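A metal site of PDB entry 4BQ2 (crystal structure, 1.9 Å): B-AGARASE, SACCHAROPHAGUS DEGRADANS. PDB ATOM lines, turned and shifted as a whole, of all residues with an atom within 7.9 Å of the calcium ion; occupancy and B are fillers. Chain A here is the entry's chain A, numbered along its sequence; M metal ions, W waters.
The calcium ion is bound by water W1 (2.1 Å), O of Lys 38 (2.3 Å), O of Asp 7 (2.3 Å), OE2 of Glu 9 (2.4 Å), OD2 of Asp 185 (2.5 Å), OD1 of Asp 185 (2.6 Å) and OG of Ser 37 (2.6 Å).
Five residues have an atom within 4 Å of the calcium ion: Asp 7, Glu 9, Ser 37, Lys 38 and Asp 185.
The backbone NH (N) of Ser 37 is in hydrogen-bond range of the backbone carbonyl oxygen (O) of Tyr 29, 2.9 Å away.
OH of Tyr 29 lies close to OD2 of Asp 185 (2.5 Å).
The backbone carbonyl oxygen (O) of Asp 185 lies within hydrogen-bond range of the backbone NH (N) of Asp 75.
OD1 of Asp 185 sits close to OD1 of Asn 186 (3.4 Å).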
ATOM      1  N   MET A   4      26.733  12.828 -16.554  1.00  0.00           N
ATOM      2  CA  MET A   4      25.409  13.307 -16.194  1.00  0.00           C
ATOM      3  C   MET A   4      24.472  12.146 -15.839  1.00  0.00           C
ATOM      4  O   MET A   4      24.312  11.204 -16.614  1.00  0.00           O
ATOM      5  CB  MET A   4      24.809  14.203 -17.304  1.00  0.00           C
ATOM      6  CG  MET A   4      23.428  14.767 -17.013  1.00  0.00           C
ATOM      7  SD  MET A   4      23.328  15.836 -15.545  1.00  0.00           S
ATOM      8  CE  MET A   4      24.336  17.182 -16.131  1.00  0.00           C
ATOM      9  N   PHE A   6      21.001  12.817 -14.168  1.00  0.00           N
ATOM     10  CA  PHE A   6      19.638  13.314 -14.412  1.00  0.00           C
ATOM     11  C   PHE A   6      19.673  14.815 -14.639  1.00  0.00           C
ATOM     12  O   PHE A   6      19.939  15.577 -13.706  1.00  0.00           O
ATOM     13  CB  PHE A   6      18.700  13.034 -13.204  1.00  0.00           C
ATOM     14  CG  PHE A   6      18.552  11.579 -12.878  1.00  0.00           C
ATOM     15  CD1 PHE A   6      17.596  10.775 -13.533  1.00  0.00           C
ATOM     16  CD2 PHE A   6      19.408  10.970 -11.957  1.00  0.00           C
ATOM     17  CE1 PHE A   6      17.479   9.420 -13.248  1.00  0.00           C
ATOM     18  CE2 PHE A   6      19.299   9.603 -11.671  1.00  0.00           C
ATOM     19  CZ  PHE A   6      18.328   8.833 -12.308  1.00  0.00           C
ATOM     20  N   ASP A   7      19.377  15.248 -15.871  1.00  0.00           N
ATOM     21  CA  ASP A   7      19.211  16.687 -16.135  1.00  0.00           C
ATOM     22  C   ASP A   7      17.763  17.081 -16.380  1.00  0.00           C
ATOM     23  O   ASP A   7      17.468  18.251 -16.579  1.00  0.00           O
ATOM     24  CB  ASP A   7      20.108  17.189 -17.283  1.00  0.00           C
ATOM     25  CG  ASP A   7      19.782  16.572 -18.637  1.00  0.00           C
ATOM     26  OD1 ASP A   7      18.695  16.006 -18.870  1.00  0.00           O
ATOM     27  OD2 ASP A   7      20.657  16.649 -19.498  1.00  0.00           O
ATOM     28  N   PHE A   8      16.874  16.073 -16.364  1.00  0.00           N
ATOM     29  CA  PHE A   8      15.403  16.260 -16.510  1.00  0.00           C
ATOM     30  C   PHE A   8      14.930  16.919 -17.813  1.00  0.00           C
ATOM     31  O   PHE A   8      13.768  17.345 -17.907  1.00  0.00           O
ATOM     32  CB  PHE A   8      14.805  16.924 -15.255  1.00  0.00           C
ATOM     33  CG  PHE A   8      15.202  16.231 -13.990  1.00  0.00           C
ATOM     34  CD1 PHE A   8      14.603  15.022 -13.642  1.00  0.00           C
ATOM     35  CD2 PHE A   8      16.246  16.708 -13.198  1.00  0.00           C
ATOM     36  CE1 PHE A   8      14.992  14.323 -12.495  1.00  0.00           C
ATOM     37  CE2 PHE A   8      16.640  16.012 -12.044  1.00  0.00           C
ATOM     38  CZ  PHE A   8      16.012  14.827 -11.701  1.00  0.00           C
ATOM     39  N   GLU A   9      15.808  16.960 -18.823  1.00  0.00           N
ATOM     40  CA  GLU A   9      15.508  17.682 -20.073  1.00  0.00           C
ATOM     41  C   GLU A   9      14.533  16.943 -21.012  1.00  0.00           C
ATOM     42  O   GLU A   9      13.875  17.560 -21.830  1.00  0.00           O
ATOM     43  CB  GLU A   9      16.797  18.053 -20.819  1.00  0.00           C
ATOM     44  CG  GLU A   9      17.654  19.046 -20.052  1.00  0.00           C
ATOM     45  CD  GLU A   9      16.860  20.299 -19.720  1.00  0.00           C
ATOM     46  OE1 GLU A   9      16.270  20.864 -20.656  1.00  0.00           O
ATOM     47  OE2 GLU A   9      16.778  20.696 -18.531  1.00  0.00           O
ATOM     48  N   ASN A  10      14.474  15.625 -20.917  1.00  0.00           N
ATOM     49  CA  ASN A  10      13.468  14.882 -21.684  1.00  0.00           C
ATOM     50  C   ASN A  10      12.033  15.050 -21.100  1.00  0.00           C
ATOM     51  O   ASN A  10      11.108  14.376 -21.532  1.00  0.00           O
ATOM     52  CB  ASN A  10      13.870  13.401 -21.795  1.00  0.00           C
ATOM     53  CG  ASN A  10      13.819  12.666 -20.465  1.00  0.00           C
ATOM     54  OD1 ASN A  10      13.517  13.265 -19.424  1.00  0.00           O
ATOM     55  ND2 ASN A  10      14.093  11.363 -20.492  1.00  0.00           N
ATOM     56  N   ILE A  26       8.040  17.935 -13.331  1.00  0.00           N
ATOM     57  CA  ILE A  26       9.125  18.625 -14.026  1.00  0.00           C
ATOM     58  C   ILE A  26       8.635  20.024 -14.339  1.00  0.00           C
ATOM     59  O   ILE A  26       7.571  20.202 -14.945  1.00  0.00           O
ATOM     60  CB  ILE A  26       9.549  17.922 -15.332  1.00  0.00           C
ATOM     61  CG1 ILE A  26       9.967  16.472 -15.089  1.00  0.00           C
ATOM     62  CG2 ILE A  26      10.707  18.693 -16.008  1.00  0.00           C
ATOM     63  CD1 ILE A  26      11.182  16.286 -14.207  1.00  0.00           C
ATOM     64  N   GLU A  27       9.397  21.015 -13.891  1.00  0.00           N
ATOM     65  CA  GLU A  27       9.061  22.433 -14.131  1.00  0.00           C
ATOM     66  C   GLU A  27      10.307  23.176 -14.608  1.00  0.00           C
ATOM     67  O   GLU A  27      11.445  22.720 -14.385  1.00  0.00           O
ATOM     68  CB  GLU A  27       8.578  23.131 -12.850  1.00  0.00           C
ATOM     69  CG  GLU A  27       7.611  22.363 -11.952  1.00  0.00           C
ATOM     70  CD  GLU A  27       6.190  22.289 -12.499  1.00  0.00           C
ATOM     71  OE1 GLU A  27       5.915  22.944 -13.531  1.00  0.00           O
ATOM     72  OE2 GLU A  27       5.364  21.571 -11.875  1.00  0.00           O
ATOM     73  N   TYR A  29      12.715  26.328 -14.066  1.00  0.00           N
ATOM     74  CA  TYR A  29      13.177  27.139 -12.910  1.00  0.00           C
ATOM     75  C   TYR A  29      14.470  27.817 -13.410  1.00  0.00           C
ATOM     76  O   TYR A  29      15.033  27.368 -14.428  1.00  0.00           O
ATOM     77  CB  TYR A  29      13.475  26.220 -11.706  1.00  0.00           C
ATOM     78  CG  TYR A  29      14.808  25.532 -11.923  1.00  0.00           C
ATOM     79  CD1 TYR A  29      14.916  24.456 -12.813  1.00  0.00           C
ATOM     80  CD2 TYR A  29      15.957  26.000 -11.330  1.00  0.00           C
ATOM     81  CE1 TYR A  29      16.143  23.859 -13.057  1.00  0.00           C
ATOM     82  CE2 TYR A  29      17.196  25.425 -11.593  1.00  0.00           C
ATOM     83  CZ  TYR A  29      17.278  24.351 -12.467  1.00  0.00           C
ATOM     84  OH  TYR A  29      18.496  23.788 -12.735  1.00  0.00           O
ATOM     85  N   GLU A  35      20.392  30.615 -16.111  1.00  0.00           N
ATOM     86  CA  GLU A  35      19.547  30.179 -17.220  1.00  0.00           C
ATOM     87  C   GLU A  35      18.411  29.225 -16.788  1.00  0.00           C
ATOM     88  O   GLU A  35      18.669  28.249 -16.076  1.00  0.00           O
ATOM     89  CB  GLU A  35      20.386  29.440 -18.259  1.00  0.00           C
ATOM     90  CG  GLU A  35      21.632  30.182 -18.736  1.00  0.00           C
ATOM     91  CD  GLU A  35      22.398  29.375 -19.749  1.00  0.00           C
ATOM     92  OE1 GLU A  35      21.817  28.444 -20.335  1.00  0.00           O
ATOM     93  OE2 GLU A  35      23.580  29.639 -19.963  1.00  0.00           O
ATOM     94  N   PRO A  36      17.193  29.484 -17.287  1.00  0.00           N
ATOM     95  CA  PRO A  36      16.077  28.561 -17.045  1.00  0.00           C
ATOM     96  C   PRO A  36      16.413  27.157 -17.556  1.00  0.00           C
ATOM     97  O   PRO A  36      17.097  26.985 -18.562  1.00  0.00           O
ATOM     98  CB  PRO A  36      14.943  29.154 -17.877  1.00  0.00           C
ATOM     99  CG  PRO A  36      15.244  30.597 -17.975  1.00  0.00           C
ATOM    100  CD  PRO A  36      16.745  30.751 -17.892  1.00  0.00           C
ATOM    101  N   SER A  37      15.928  26.149 -16.854  1.00  0.00           N
ATOM    102  CA  SER A  37      16.213  24.783 -17.224  1.00  0.00           C
ATOM    103  C   SER A  37      15.051  23.963 -16.700  1.00  0.00           C
ATOM    104  O   SER A  37      14.332  24.443 -15.854  1.00  0.00           O
ATOM    105  CB  SER A  37      17.506  24.326 -16.567  1.00  0.00           C
ATOM    106  OG  SER A  37      17.933  23.071 -17.076  1.00  0.00           O
ATOM    107  N   LYS A  38      14.840  22.760 -17.210  1.00  0.00           N
ATOM    108  CA  LYS A  38      13.862  21.870 -16.601  1.00  0.00           C
ATOM    109  C   LYS A  38      14.448  21.202 -15.350  1.00  0.00           C
ATOM    110  O   LYS A  38      15.532  20.638 -15.422  1.00  0.00           O
ATOM    111  CB  LYS A  38      13.418  20.799 -17.597  1.00  0.00           C
ATOM    112  CG  LYS A  38      12.851  21.324 -18.895  1.00  0.00           C
ATOM    113  CD  LYS A  38      11.369  21.552 -18.864  1.00  0.00           C
ATOM    114  CE  LYS A  38      10.762  21.210 -20.225  1.00  0.00           C
ATOM    115  NZ  LYS A  38      11.714  21.364 -21.345  1.00  0.00           N
ATOM    116  N   GLY A  39      13.725  21.259 -14.228  1.00  0.00           N
ATOM    117  CA  GLY A  39      14.174  20.612 -12.992  1.00  0.00           C
ATOM    118  C   GLY A  39      13.072  19.747 -12.370  1.00  0.00           C
ATOM    119  O   GLY A  39      11.913  19.798 -12.770  1.00  0.00           O
ATOM    120  N   LEU A  40      13.466  18.917 -11.418  1.00  0.00           N
ATOM    121  CA  LEU A  40      12.515  18.115 -10.665  1.00  0.00           C
ATOM    122  C   LEU A  40      12.022  18.900  -9.456  1.00  0.00           C
ATOM    123  O   LEU A  40      12.805  19.184  -8.515  1.00  0.00           O
ATOM    124  CB  LEU A  40      13.156  16.823 -10.204  1.00  0.00           C
ATOM    125  CG  LEU A  40      12.211  15.893  -9.408  1.00  0.00           C
ATOM    126  CD1 LEU A  40      11.271  15.152 -10.343  1.00  0.00           C
ATOM    127  CD2 LEU A  40      13.100  14.923  -8.655  1.00  0.00           C
ATOM    128  N   ASP A  75      22.192  20.207  -8.133  1.00  0.00           N
ATOM    129  CA  ASP A  75      21.781  21.613  -8.057  1.00  0.00           C
ATOM    130  C   ASP A  75      20.441  21.618  -7.328  1.00  0.00           C
ATOM    131  O   ASP A  75      19.547  20.853  -7.688  1.00  0.00           O
ATOM    132  CB  ASP A  75      21.615  22.265  -9.444  1.00  0.00           C
ATOM    133  CG  ASP A  75      22.917  22.338 -10.248  1.00  0.00           C
ATOM    134  OD1 ASP A  75      24.007  22.003  -9.712  1.00  0.00           O
ATOM    135  OD2 ASP A  75      22.824  22.666 -11.454  1.00  0.00           O
ATOM    136  N   ILE A 184      15.328  20.290  -7.886  1.00  0.00           N
ATOM    137  CA  ILE A 184      16.590  19.557  -8.014  1.00  0.00           C
ATOM    138  C   ILE A 184      16.905  19.473  -9.516  1.00  0.00           C
ATOM    139  O   ILE A 184      16.008  19.229 -10.330  1.00  0.00           O
ATOM    140  CB  ILE A 184      16.466  18.147  -7.433  1.00  0.00           C
ATOM    141  CG1 ILE A 184      16.167  18.185  -5.906  1.00  0.00           C
ATOM    142  CG2 ILE A 184      17.719  17.318  -7.738  1.00  0.00           C
ATOM    143  CD1 ILE A 184      15.719  16.846  -5.338  1.00  0.00           C
ATOM    144  N   ASP A 185      18.167  19.673  -9.889  1.00  0.00           N
ATOM    145  CA  ASP A 185      18.565  19.540 -11.293  1.00  0.00           C
ATOM    146  C   ASP A 185      19.996  19.084 -11.375  1.00  0.00           C
ATOM    147  O   ASP A 185      20.766  19.236 -10.404  1.00  0.00           O
ATOM    148  CB  ASP A 185      18.307  20.875 -12.021  1.00  0.00           C
ATOM    149  CG  ASP A 185      18.326  20.729 -13.541  1.00  0.00           C
ATOM    150  OD1 ASP A 185      18.452  19.587 -14.045  1.00  0.00           O
ATOM    151  OD2 ASP A 185      18.268  21.757 -14.236  1.00  0.00           O
ATOM    152  N   ASN A 186      20.364  18.460 -12.508  1.00  0.00           N
ATOM    153  CA  ASN A 186      21.749  18.170 -12.866  1.00  0.00           C
ATOM    154  C   ASN A 186      22.444  17.230 -11.896  1.00  0.00           C
ATOM    155  O   ASN A 186      23.541  17.513 -11.424  1.00  0.00           O
ATOM    156  CB  ASN A 186      22.555  19.463 -13.052  1.00  0.00           C
ATOM    157  CG  ASN A 186      21.978  20.333 -14.164  1.00  0.00           C
ATOM    158  OD1 ASN A 186      21.638  19.822 -15.244  1.00  0.00           O
ATOM    159  ND2 ASN A 186      21.855  21.638 -13.927  1.00  0.00           N
ATOM    160  N   ILE A 187      21.771  16.151 -11.537  1.00  0.00           N
ATOM    161  CA  ILE A 187      22.390  15.158 -10.723  1.00  0.00           C
ATOM    162  C   ILE A 187      23.500  14.523 -11.547  1.00  0.00           C
ATOM    163  O   ILE A 187      23.255  13.948 -12.617  1.00  0.00           O
ATOM    164  CB  ILE A 187      21.384  14.098 -10.244  1.00  0.00           C
ATOM    165  CG1 ILE A 187      20.151  14.804  -9.656  1.00  0.00           C
ATOM    166  CG2 ILE A 187      22.096  13.184  -9.284  1.00  0.00           C
ATOM    167  CD1 ILE A 187      19.123  13.923  -8.959  1.00  0.00           C
HETATM  168 CA    CA M   1      17.650  20.552 -16.336  1.00  0.00          CA
HETATM  169  O   HOH W   1      19.558  20.743 -17.175  1.00  0.00           O
